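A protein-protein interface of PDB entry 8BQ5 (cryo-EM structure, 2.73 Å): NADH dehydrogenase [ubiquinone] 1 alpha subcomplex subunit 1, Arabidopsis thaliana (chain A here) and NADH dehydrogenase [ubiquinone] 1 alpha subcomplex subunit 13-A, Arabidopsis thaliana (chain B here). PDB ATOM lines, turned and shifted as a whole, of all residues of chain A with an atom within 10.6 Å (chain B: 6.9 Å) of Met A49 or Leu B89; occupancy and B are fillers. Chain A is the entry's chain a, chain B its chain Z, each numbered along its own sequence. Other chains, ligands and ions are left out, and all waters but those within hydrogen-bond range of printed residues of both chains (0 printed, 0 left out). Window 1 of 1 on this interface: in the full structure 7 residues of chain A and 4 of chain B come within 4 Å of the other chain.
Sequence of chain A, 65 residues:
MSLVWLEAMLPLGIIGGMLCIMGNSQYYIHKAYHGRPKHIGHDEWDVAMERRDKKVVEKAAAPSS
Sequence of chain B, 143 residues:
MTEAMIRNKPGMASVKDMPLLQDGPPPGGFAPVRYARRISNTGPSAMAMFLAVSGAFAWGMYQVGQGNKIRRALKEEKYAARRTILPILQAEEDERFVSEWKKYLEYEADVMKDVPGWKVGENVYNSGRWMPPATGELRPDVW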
ATOM      1  N   ARG A  36      -6.993  15.992 -18.304  1.00  0.00           N
ATOM      2  CA  ARG A  36      -7.878  15.091 -17.585  1.00  0.00           C
ATOM      3  C   ARG A  36      -9.234  15.762 -17.429  1.00  0.00           C
ATOM      4  O   ARG A  36      -9.333  16.992 -17.488  1.00  0.00           O
ATOM      5  CB  ARG A  36      -7.307  14.712 -16.210  1.00  0.00           C
ATOM      6  CG  ARG A  36      -6.685  15.858 -15.430  1.00  0.00           C
ATOM      7  CD  ARG A  36      -6.085  15.354 -14.125  1.00  0.00           C
ATOM      8  NE  ARG A  36      -5.385  16.401 -13.391  1.00  0.00           N
ATOM      9  CZ  ARG A  36      -4.821  16.234 -12.203  1.00  0.00           C
ATOM     10  NH1 ARG A  36      -4.861  15.070 -11.577  1.00  0.00           N
ATOM     11  NH2 ARG A  36      -4.203  17.261 -11.628  1.00  0.00           N
ATOM     12  N   HIS A  39     -12.701  17.760 -12.305  1.00  0.00           N
ATOM     13  CA  HIS A  39     -12.968  17.122 -11.024  1.00  0.00           C
ATOM     14  C   HIS A  39     -14.007  17.932 -10.260  1.00  0.00           C
ATOM     15  O   HIS A  39     -13.825  19.136 -10.045  1.00  0.00           O
ATOM     16  CB  HIS A  39     -11.682  16.997 -10.207  1.00  0.00           C
ATOM     17  CG  HIS A  39     -11.862  16.291  -8.899  1.00  0.00           C
ATOM     18  ND1 HIS A  39     -11.253  16.713  -7.738  1.00  0.00           N
ATOM     19  CD2 HIS A  39     -12.578  15.190  -8.570  1.00  0.00           C
ATOM     20  CE1 HIS A  39     -11.589  15.904  -6.749  1.00  0.00           C
ATOM     21  NE2 HIS A  39     -12.392  14.972  -7.228  1.00  0.00           N
ATOM     22  N   HIS A  42     -13.322  20.179  -6.216  1.00  0.00           N
ATOM     23  CA  HIS A  42     -11.954  20.662  -6.062  1.00  0.00           C
ATOM     24  C   HIS A  42     -11.884  21.631  -4.888  1.00  0.00           C
ATOM     25  O   HIS A  42     -12.386  22.755  -4.973  1.00  0.00           O
ATOM     26  CB  HIS A  42     -11.504  21.339  -7.353  1.00  0.00           C
ATOM     27  CG  HIS A  42     -10.112  20.989  -7.771  1.00  0.00           C
ATOM     28  ND1 HIS A  42      -9.741  19.711  -8.131  1.00  0.00           N
ATOM     29  CD2 HIS A  42      -9.003  21.754  -7.901  1.00  0.00           C
ATOM     30  CE1 HIS A  42      -8.461  19.703  -8.458  1.00  0.00           C
ATOM     31  NE2 HIS A  42      -7.990  20.931  -8.327  1.00  0.00           N
ATOM     32  N   ASP A  43     -11.250  21.208  -3.797  1.00  0.00           N
ATOM     33  CA  ASP A  43     -11.189  21.996  -2.576  1.00  0.00           C
ATOM     34  C   ASP A  43      -9.766  22.500  -2.343  1.00  0.00           C
ATOM     35  O   ASP A  43      -8.890  22.377  -3.206  1.00  0.00           O
ATOM     36  CB  ASP A  43     -11.714  21.182  -1.387  1.00  0.00           C
ATOM     37  CG  ASP A  43     -11.063  19.814  -1.264  1.00  0.00           C
ATOM     38  OD1 ASP A  43      -9.882  19.658  -1.641  1.00  0.00           O
ATOM     39  OD2 ASP A  43     -11.740  18.887  -0.774  1.00  0.00           O
ATOM     40  N   GLU A  44      -9.548  23.097  -1.167  1.00  0.00           N
ATOM     41  CA  GLU A  44      -8.225  23.610  -0.817  1.00  0.00           C
ATOM     42  C   GLU A  44      -7.164  22.521  -0.927  1.00  0.00           C
ATOM     43  O   GLU A  44      -6.039  22.780  -1.375  1.00  0.00           O
ATOM     44  CB  GLU A  44      -8.238  24.188   0.600  1.00  0.00           C
ATOM     45  CG  GLU A  44      -8.958  25.522   0.769  1.00  0.00           C
ATOM     46  CD  GLU A  44     -10.437  25.449   0.435  1.00  0.00           C
ATOM     47  OE1 GLU A  44     -11.118  24.521   0.912  1.00  0.00           O
ATOM     48  OE2 GLU A  44     -10.922  26.328  -0.299  1.00  0.00           O
ATOM     49  N   TRP A  45      -7.505  21.296  -0.524  1.00  0.00           N
ATOM     50  CA  TRP A  45      -6.542  20.200  -0.559  1.00  0.00           C
ATOM     51  C   TRP A  45      -6.161  19.841  -1.989  1.00  0.00           C
ATOM     52  O   TRP A  45      -4.981  19.640  -2.293  1.00  0.00           O
ATOM     53  CB  TRP A  45      -7.109  18.981   0.167  1.00  0.00           C
ATOM     54  CG  TRP A  45      -6.175  17.810   0.192  1.00  0.00           C
ATOM     55  CD1 TRP A  45      -6.014  16.869  -0.783  1.00  0.00           C
ATOM     56  CD2 TRP A  45      -5.276  17.454   1.247  1.00  0.00           C
ATOM     57  NE1 TRP A  45      -5.069  15.950  -0.400  1.00  0.00           N
ATOM     58  CE2 TRP A  45      -4.600  16.287   0.841  1.00  0.00           C
ATOM     59  CE3 TRP A  45      -4.976  18.008   2.494  1.00  0.00           C
ATOM     60  CZ2 TRP A  45      -3.644  15.664   1.639  1.00  0.00           C
ATOM     61  CZ3 TRP A  45      -4.027  17.389   3.283  1.00  0.00           C
ATOM     62  CH2 TRP A  45      -3.371  16.231   2.853  1.00  0.00           C
ATOM     63  N   ASP A  46      -7.149  19.737  -2.882  1.00  0.00           N
ATOM     64  CA  ASP A  46      -6.852  19.413  -4.275  1.00  0.00           C
ATOM     65  C   ASP A  46      -6.001  20.499  -4.923  1.00  0.00           C
ATOM     66  O   ASP A  46      -5.076  20.200  -5.690  1.00  0.00           O
ATOM     67  CB  ASP A  46      -8.150  19.202  -5.055  1.00  0.00           C
ATOM     68  CG  ASP A  46      -8.882  17.938  -4.645  1.00  0.00           C
ATOM     69  OD1 ASP A  46      -8.235  16.874  -4.551  1.00  0.00           O
ATOM     70  OD2 ASP A  46     -10.105  18.008  -4.410  1.00  0.00           O
ATOM     71  N   VAL A  47      -6.267  21.762  -4.598  1.00  0.00           N
ATOM     72  CA  VAL A  47      -5.452  22.884  -5.150  1.00  0.00           C
ATOM     73  C   VAL A  47      -4.009  22.788  -4.634  1.00  0.00           C
ATOM     74  O   VAL A  47      -3.092  22.865  -5.465  1.00  0.00           O
ATOM     75  CB  VAL A  47      -6.112  24.239  -4.832  1.00  0.00           C
ATOM     76  CG1 VAL A  47      -5.184  25.413  -5.080  1.00  0.00           C
ATOM     77  CG2 VAL A  47      -7.409  24.406  -5.606  1.00  0.00           C
ATOM     78  N   ALA A  48      -3.815  22.609  -3.327  1.00  0.00           N
ATOM     79  CA  ALA A  48      -2.465  22.470  -2.731  1.00  0.00           C
ATOM     80  C   ALA A  48      -1.714  21.313  -3.400  1.00  0.00           C
ATOM     81  O   ALA A  48      -0.531  21.495  -3.715  1.00  0.00           O
ATOM     82  CB  ALA A  48      -2.589  22.263  -1.245  1.00  0.00           C
ATOM     83  N   MET A  49      -2.394  20.198  -3.655  1.00  0.00           N
ATOM     84  CA  MET A  49      -1.765  19.021  -4.310  1.00  0.00           C
ATOM     85  C   MET A  49      -1.275  19.405  -5.707  1.00  0.00           C
ATOM     86  O   MET A  49      -0.109  19.155  -5.983  1.00  0.00           O
ATOM     87  CB  MET A  49      -2.766  17.871  -4.426  1.00  0.00           C
ATOM     88  CG  MET A  49      -3.022  17.138  -3.130  1.00  0.00           C
ATOM     89  SD  MET A  49      -1.539  16.930  -2.130  1.00  0.00           S
ATOM     90  CE  MET A  49      -1.908  18.041  -0.777  1.00  0.00           C
ATOM     91  N   GLU A  50      -2.140  19.993  -6.534  1.00  0.00           N
ATOM     92  CA  GLU A  50      -1.787  20.378  -7.925  1.00  0.00           C
ATOM     93  C   GLU A  50      -0.549  21.282  -7.952  1.00  0.00           C
ATOM     94  O   GLU A  50       0.347  21.018  -8.771  1.00  0.00           O
ATOM     95  CB  GLU A  50      -2.967  21.107  -8.553  1.00  0.00           C
ATOM     96  CG  GLU A  50      -3.954  20.185  -9.245  1.00  0.00           C
ATOM     97  CD  GLU A  50      -4.978  20.892 -10.116  1.00  0.00           C
ATOM     98  OE1 GLU A  50      -5.812  20.194 -10.724  1.00  0.00           O
ATOM     99  OE2 GLU A  50      -4.944  22.140 -10.183  1.00  0.00           O
ATOM    100  N   ARG A  51      -0.515  22.310  -7.113  1.00  0.00           N
ATOM    101  CA  ARG A  51       0.621  23.268  -7.104  1.00  0.00           C
ATOM    102  C   ARG A  51       1.903  22.537  -6.689  1.00  0.00           C
ATOM    103  O   ARG A  51       2.926  22.742  -7.352  1.00  0.00           O
ATOM    104  CB  ARG A  51       0.272  24.458  -6.201  1.00  0.00           C
ATOM    105  CG  ARG A  51      -0.979  25.195  -6.656  1.00  0.00           C
ATOM    106  CD  ARG A  51      -1.353  26.442  -5.875  1.00  0.00           C
ATOM    107  NE  ARG A  51      -2.477  27.092  -6.538  1.00  0.00           N
ATOM    108  CZ  ARG A  51      -3.090  28.196  -6.121  1.00  0.00           C
ATOM    109  NH1 ARG A  51      -2.695  28.808  -5.018  1.00  0.00           N
ATOM    110  NH2 ARG A  51      -4.104  28.682  -6.813  1.00  0.00           N
ATOM    111  N   ARG A  52       1.836  21.715  -5.642  1.00  0.00           N
ATOM    112  CA  ARG A  52       3.016  20.950  -5.157  1.00  0.00           C
ATOM    113  C   ARG A  52       3.434  19.936  -6.226  1.00  0.00           C
ATOM    114  O   ARG A  52       4.631  19.876  -6.516  1.00  0.00           O
ATOM    115  CB  ARG A  52       2.673  20.292  -3.820  1.00  0.00           C
ATOM    116  CG  ARG A  52       3.679  19.259  -3.347  1.00  0.00           C
ATOM    117  CD  ARG A  52       3.029  17.910  -3.160  1.00  0.00           C
ATOM    118  NE  ARG A  52       4.038  16.930  -2.797  1.00  0.00           N
ATOM    119  CZ  ARG A  52       4.064  15.680  -3.235  1.00  0.00           C
ATOM    120  NH1 ARG A  52       3.131  15.245  -4.066  1.00  0.00           N
ATOM    121  NH2 ARG A  52       5.030  14.869  -2.844  1.00  0.00           N
ATOM    122  N   ASP A  53       2.486  19.204  -6.814  1.00  0.00           N
ATOM    123  CA  ASP A  53       2.791  18.253  -7.916  1.00  0.00           C
ATOM    124  C   ASP A  53       3.524  18.961  -9.051  1.00  0.00           C
ATOM    125  O   ASP A  53       4.471  18.376  -9.552  1.00  0.00           O
ATOM    126  CB  ASP A  53       1.534  17.585  -8.465  1.00  0.00           C
ATOM    127  CG  ASP A  53       1.160  16.327  -7.715  1.00  0.00           C
ATOM    128  OD1 ASP A  53       0.615  15.414  -8.358  1.00  0.00           O
ATOM    129  OD2 ASP A  53       1.420  16.273  -6.497  1.00  0.00           O
ATOM    130  N   LYS A  54       3.101  20.170  -9.427  1.00  0.00           N
ATOM    131  CA  LYS A  54       3.817  20.940 -10.477  1.00  0.00           C
ATOM    132  C   LYS A  54       5.314  20.984 -10.132  1.00  0.00           C
ATOM    133  O   LYS A  54       6.099  20.555 -10.978  1.00  0.00           O
ATOM    134  CB  LYS A  54       3.200  22.332 -10.630  1.00  0.00           C
ATOM    135  CG  LYS A  54       1.783  22.356 -11.183  1.00  0.00           C
ATOM    136  CD  LYS A  54       1.215  23.751 -11.291  1.00  0.00           C
ATOM    137  CE  LYS A  54      -0.186  23.779 -11.863  1.00  0.00           C
ATOM    138  NZ  LYS A  54      -0.725  25.157 -11.934  1.00  0.00           N
ATOM    139  N   LYS A  55       5.687  21.474  -8.942  1.00  0.00           N
ATOM    140  CA  LYS A  55       7.117  21.435  -8.521  1.00  0.00           C
ATOM    141  C   LYS A  55       7.631  19.990  -8.541  1.00  0.00           C
ATOM    142  O   LYS A  55       8.652  19.748  -9.192  1.00  0.00           O
ATOM    143  CB  LYS A  55       7.305  21.962  -7.098  1.00  0.00           C
ATOM    144  CG  LYS A  55       6.365  23.079  -6.667  1.00  0.00           C
ATOM    145  CD  LYS A  55       6.408  23.324  -5.175  1.00  0.00           C
ATOM    146  CE  LYS A  55       5.304  24.235  -4.684  1.00  0.00           C
ATOM    147  NZ  LYS A  55       4.658  23.706  -3.460  1.00  0.00           N
ATOM    148  N   VAL A  56       6.924  19.059  -7.893  1.00  0.00           N
ATOM    149  CA  VAL A  56       7.411  17.689  -7.777  1.00  0.00           C
ATOM    150  C   VAL A  56       7.676  17.072  -9.146  1.00  0.00           C
ATOM    151  O   VAL A  56       8.576  16.234  -9.286  1.00  0.00           O
ATOM    152  CB  VAL A  56       6.405  16.860  -6.947  1.00  0.00           C
ATOM    153  CG1 VAL A  56       6.666  15.369  -7.074  1.00  0.00           C
ATOM    154  CG2 VAL A  56       6.461  17.283  -5.487  1.00  0.00           C
ATOM    155  N   VAL A  57       6.942  17.495 -10.172  1.00  0.00           N
ATOM    156  CA  VAL A  57       7.148  16.993 -11.525  1.00  0.00           C
ATOM    157  C   VAL A  57       8.246  17.786 -12.223  1.00  0.00           C
ATOM    158  O   VAL A  57       9.203  17.203 -12.747  1.00  0.00           O
ATOM    159  CB  VAL A  57       5.841  17.037 -12.338  1.00  0.00           C
ATOM    160  CG1 VAL A  57       6.115  16.697 -13.793  1.00  0.00           C
ATOM    161  CG2 VAL A  57       4.819  16.074 -11.754  1.00  0.00           C
ATOM    162  N   GLU A  58       8.125  19.119 -12.239  1.00  0.00           N
ATOM    163  CA  GLU A  58       9.018  19.923 -13.069  1.00  0.00           C
ATOM    164  C   GLU A  58      10.448  19.923 -12.538  1.00  0.00           C
ATOM    165  O   GLU A  58      11.405  19.990 -13.318  1.00  0.00           O
ATOM    166  CB  GLU A  58       8.482  21.351 -13.184  1.00  0.00           C
ATOM    167  CG  GLU A  58       9.341  22.262 -14.045  1.00  0.00           C
ATOM    168  CD  GLU A  58       8.593  23.486 -14.527  1.00  0.00           C
ATOM    169  OE1 GLU A  58       7.658  23.930 -13.831  1.00  0.00           O
ATOM    170  OE2 GLU A  58       8.952  24.011 -15.602  1.00  0.00           O
ATOM    171  N   ARG B  82      -6.442  11.159   3.076  1.00  0.00           N
ATOM    172  CA  ARG B  82      -5.719  12.415   3.245  1.00  0.00           C
ATOM    173  C   ARG B  82      -4.900  12.429   4.530  1.00  0.00           C
ATOM    174  O   ARG B  82      -3.841  13.063   4.583  1.00  0.00           O
ATOM    175  CB  ARG B  82      -6.695  13.586   3.227  1.00  0.00           C
ATOM    176  CG  ARG B  82      -7.055  14.026   1.830  1.00  0.00           C
ATOM    177  CD  ARG B  82      -8.204  14.997   1.829  1.00  0.00           C
ATOM    178  NE  ARG B  82      -8.574  15.362   0.469  1.00  0.00           N
ATOM    179  CZ  ARG B  82      -9.491  16.268   0.161  1.00  0.00           C
ATOM    180  NH1 ARG B  82     -10.158  16.921   1.096  1.00  0.00           N
ATOM    181  NH2 ARG B  82      -9.742  16.525  -1.119  1.00  0.00           N
ATOM    182  N   ILE B  85      -1.285  10.383   4.379  1.00  0.00           N
ATOM    183  CA  ILE B  85      -0.213  10.963   3.581  1.00  0.00           C
ATOM    184  C   ILE B  85       0.084  12.402   3.967  1.00  0.00           C
ATOM    185  O   ILE B  85       0.946  13.035   3.345  1.00  0.00           O
ATOM    186  CB  ILE B  85      -0.532  10.864   2.076  1.00  0.00           C
ATOM    187  CG1 ILE B  85      -1.768  11.694   1.727  1.00  0.00           C
ATOM    188  CG2 ILE B  85      -0.741   9.418   1.675  1.00  0.00           C
ATOM    189  CD1 ILE B  85      -1.835  12.093   0.270  1.00  0.00           C
ATOM    190  N   LEU B  86      -0.606  12.940   4.971  1.00  0.00           N
ATOM    191  CA  LEU B  86      -0.305  14.291   5.441  1.00  0.00           C
ATOM    192  C   LEU B  86       1.118  14.440   5.965  1.00  0.00           C
ATOM    193  O   LEU B  86       1.755  15.459   5.652  1.00  0.00           O
ATOM    194  CB  LEU B  86      -1.331  14.713   6.501  1.00  0.00           C
ATOM    195  CG  LEU B  86      -1.286  16.152   7.027  1.00  0.00           C
ATOM    196  CD1 LEU B  86      -2.676  16.617   7.379  1.00  0.00           C
ATOM    197  CD2 LEU B  86      -0.386  16.293   8.246  1.00  0.00           C
ATOM    198  N   PRO B  87       1.658  13.526   6.786  1.00  0.00           N
ATOM    199  CA  PRO B  87       2.999  13.775   7.347  1.00  0.00           C
ATOM    200  C   PRO B  87       4.101  13.952   6.314  1.00  0.00           C
ATOM    201  O   PRO B  87       4.967  14.809   6.510  1.00  0.00           O
ATOM    202  CB  PRO B  87       3.233  12.546   8.233  1.00  0.00           C
ATOM    203  CG  PRO B  87       1.874  12.137   8.638  1.00  0.00           C
ATOM    204  CD  PRO B  87       1.030  12.352   7.422  1.00  0.00           C
ATOM    205  N   ILE B  88       4.103  13.190   5.217  1.00  0.00           N
ATOM    206  CA  ILE B  88       5.174  13.351   4.235  1.00  0.00           C
ATOM    207  C   ILE B  88       5.053  14.696   3.522  1.00  0.00           C
ATOM    208  O   ILE B  88       6.056  15.389   3.294  1.00  0.00           O
ATOM    209  CB  ILE B  88       5.195  12.170   3.243  1.00  0.00           C
ATOM    210  CG1 ILE B  88       6.339  12.348   2.242  1.00  0.00           C
ATOM    211  CG2 ILE B  88       3.858  12.002   2.540  1.00  0.00           C
ATOM    212  CD1 ILE B  88       6.326  11.363   1.101  1.00  0.00           C
ATOM    213  N   LEU B  89       3.825  15.095   3.179  1.00  0.00           N
ATOM    214  CA  LEU B  89       3.609  16.404   2.573  1.00  0.00           C
ATOM    215  C   LEU B  89       4.052  17.520   3.510  1.00  0.00           C
ATOM    216  O   LEU B  89       4.722  18.471   3.088  1.00  0.00           O
ATOM    217  CB  LEU B  89       2.134  16.568   2.209  1.00  0.00           C
ATOM    218  CG  LEU B  89       1.560  15.549   1.226  1.00  0.00           C
ATOM    219  CD1 LEU B  89       0.046  15.502   1.326  1.00  0.00           C
ATOM    220  CD2 LEU B  89       1.992  15.889  -0.184  1.00  0.00           C
ATOM    221  N   GLN B  90       3.695  17.409   4.791  1.00  0.00           N
ATOM    222  CA  GLN B  90       4.084  18.420   5.767  1.00  0.00           C
ATOM    223  C   GLN B  90       5.595  18.469   5.940  1.00  0.00           C
ATOM    224  O   GLN B  90       6.170  19.551   6.079  1.00  0.00           O
ATOM    225  CB  GLN B  90       3.405  18.146   7.108  1.00  0.00           C
ATOM    226  CG  GLN B  90       3.243  19.374   7.988  1.00  0.00           C
ATOM    227  CD  GLN B  90       2.828  20.602   7.206  1.00  0.00           C
ATOM    228  OE1 GLN B  90       1.720  20.666   6.679  1.00  0.00           O
ATOM    229  NE2 GLN B  90       3.710  21.591   7.142  1.00  0.00           N
ATOM    230  N   ALA B  91       6.253  17.308   5.958  1.00  0.00           N
ATOM    231  CA  ALA B  91       7.704  17.280   6.103  1.00  0.00           C
ATOM    232  C   ALA B  91       8.386  17.957   4.924  1.00  0.00           C
ATOM    233  O   ALA B  91       9.328  18.744   5.103  1.00  0.00           O
ATOM    234  CB  ALA B  91       8.186  15.839   6.245  1.00  0.00           C
ATOM    235  N   GLU B  92       7.918  17.669   3.708  1.00  0.00           N
ATOM    236  CA  GLU B  92       8.478  18.321   2.531  1.00  0.00           C
ATOM    237  C   GLU B  92       8.260  19.830   2.588  1.00  0.00           C
ATOM    238  O   GLU B  92       9.167  20.614   2.280  1.00  0.00           O
ATOM    239  CB  GLU B  92       7.858  17.728   1.270  1.00  0.00           C
ATOM    240  CG  GLU B  92       7.987  18.604   0.047  1.00  0.00           C
ATOM    241  CD  GLU B  92       6.987  18.229  -1.019  1.00  0.00           C
ATOM    242  OE1 GLU B  92       5.909  18.856  -1.058  1.00  0.00           O
ATOM    243  OE2 GLU B  92       7.272  17.307  -1.810  1.00  0.00           O
ATOM    244  N   GLU B  93       7.069  20.248   3.011  1.00  0.00           N
ATOM    245  CA  GLU B  93       6.767  21.700   3.101  1.00  0.00           C
ATOM    246  C   GLU B  93       7.667  22.343   4.158  1.00  0.00           C
ATOM    247  O   GLU B  93       8.139  23.466   3.915  1.00  0.00           O
ATOM    248  CB  GLU B  93       5.282  21.923   3.403  1.00  0.00           C
ATOM    249  CG  GLU B  93       4.927  23.366   3.707  1.00  0.00           C
ATOM    250  CD  GLU B  93       5.077  24.354   2.562  1.00  0.00           C
ATOM    251  OE1 GLU B  93       5.376  25.531   2.840  1.00  0.00           O
ATOM    252  OE2 GLU B  93       4.883  23.951   1.398  1.00  0.00           O
ATOM    253  N   ASP B  94       7.895  21.657   5.276  1.00  0.00           N
ATOM    254  CA  ASP B  94       8.755  22.199   6.322  1.00  0.00           C
ATOM    255  C   ASP B  94      10.179  22.379   5.817  1.00  0.00           C
ATOM    256  O   ASP B  94      10.808  23.416   6.056  1.00  0.00           O
ATOM    257  CB  ASP B  94       8.741  21.282   7.546  1.00  0.00           C
ATOM    258  CG  ASP B  94       7.461  21.393   8.350  1.00  0.00           C
ATOM    259  OD1 ASP B  94       6.562  22.157   7.944  1.00  0.00           O
ATOM    260  OD2 ASP B  94       7.366  20.725   9.400  1.00  0.00           O
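The backbone NH of Trp A45 lies within hydrogen-bond range of the side-chain carboxylate of Asp A43, 3.1 Å away. N of Asp A46 is in hydrogen-bond range of OD1 of Asp A43 (3.0 Å). The guanidinium group (NH1) of Arg A52 is in salt-bridge range of the side-chain carboxylate (OD2) of Asp A53.
OD2 of Asp A43 lies within salt-bridge range of NH2 of Arg B82 (3.1 Å). The guanidinium group (NE) of Arg A52 is in salt-bridge range of the side-chain carboxylate (OE1) of Glu B92, at 3.2 Å. NH2 of Arg B82 is in salt-bridge range of OD2 of Asp A46.
Met A49 touches just one residue of chain B: Leu B89 (3.8 Å). No residue of chain A comes within 4 Å of Ile B85. No residue of chain A comes within 4 Å of Ile B88. No residue of chain A comes within 4 Å of Gln B90. No residue of chain A comes within 4 Å of Ala B91. Glu B92 touches just these residues of chain A: Arg A52 (3.2 Å) and Val A56 (3.8 Å). Of the printed residues of chain B, Asp A46 touches Arg B82 (3.6 Å). Of the printed residues of chain B, Trp A45 touches Arg B82 (3.2 Å) and Leu B89 (3.7 Å). Of the printed residues of chain B, Asp A43 touches Arg B82 (3.1 Å). Printed residues of chain B within 4 Å of Val A56: Glu B92 (3.8 Å).
Among the printed residues, pairs that only touch across the chains: Trp A45 with Arg B82 (3.2 Å), Trp A45 with Leu B89 (3.7 Å), Met A49 with Leu B89 (3.8 Å), Arg A52 with Leu B89 (3.5 Å) and Val A56 with Glu B92 (3.8 Å).
Of the 19 printed residues of chain A, 6 touch a printed residue of chain B. Printed residues of chain A that touch a printed residue of chain B: Asp A43, Trp A45, Asp A46, Met A49, Arg A52 and Val A56. Printed residues of chain B that touch a printed residue of chain A: Arg B82, Leu B89 and Glu B92. Hydrophobic or aromatic side chains of chain B within 4 Å of the printed part of chain A: Leu B89. Among the printed residues, Asp or Glu carboxylates within 4 Å of a Lys or Arg side-chain nitrogen of the other chain: Asp A43 with Arg B82 (3.1 Å), Asp A46 with Arg B82 (3.6 Å) and Arg A52 with Glu B92 (3.2 Å).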
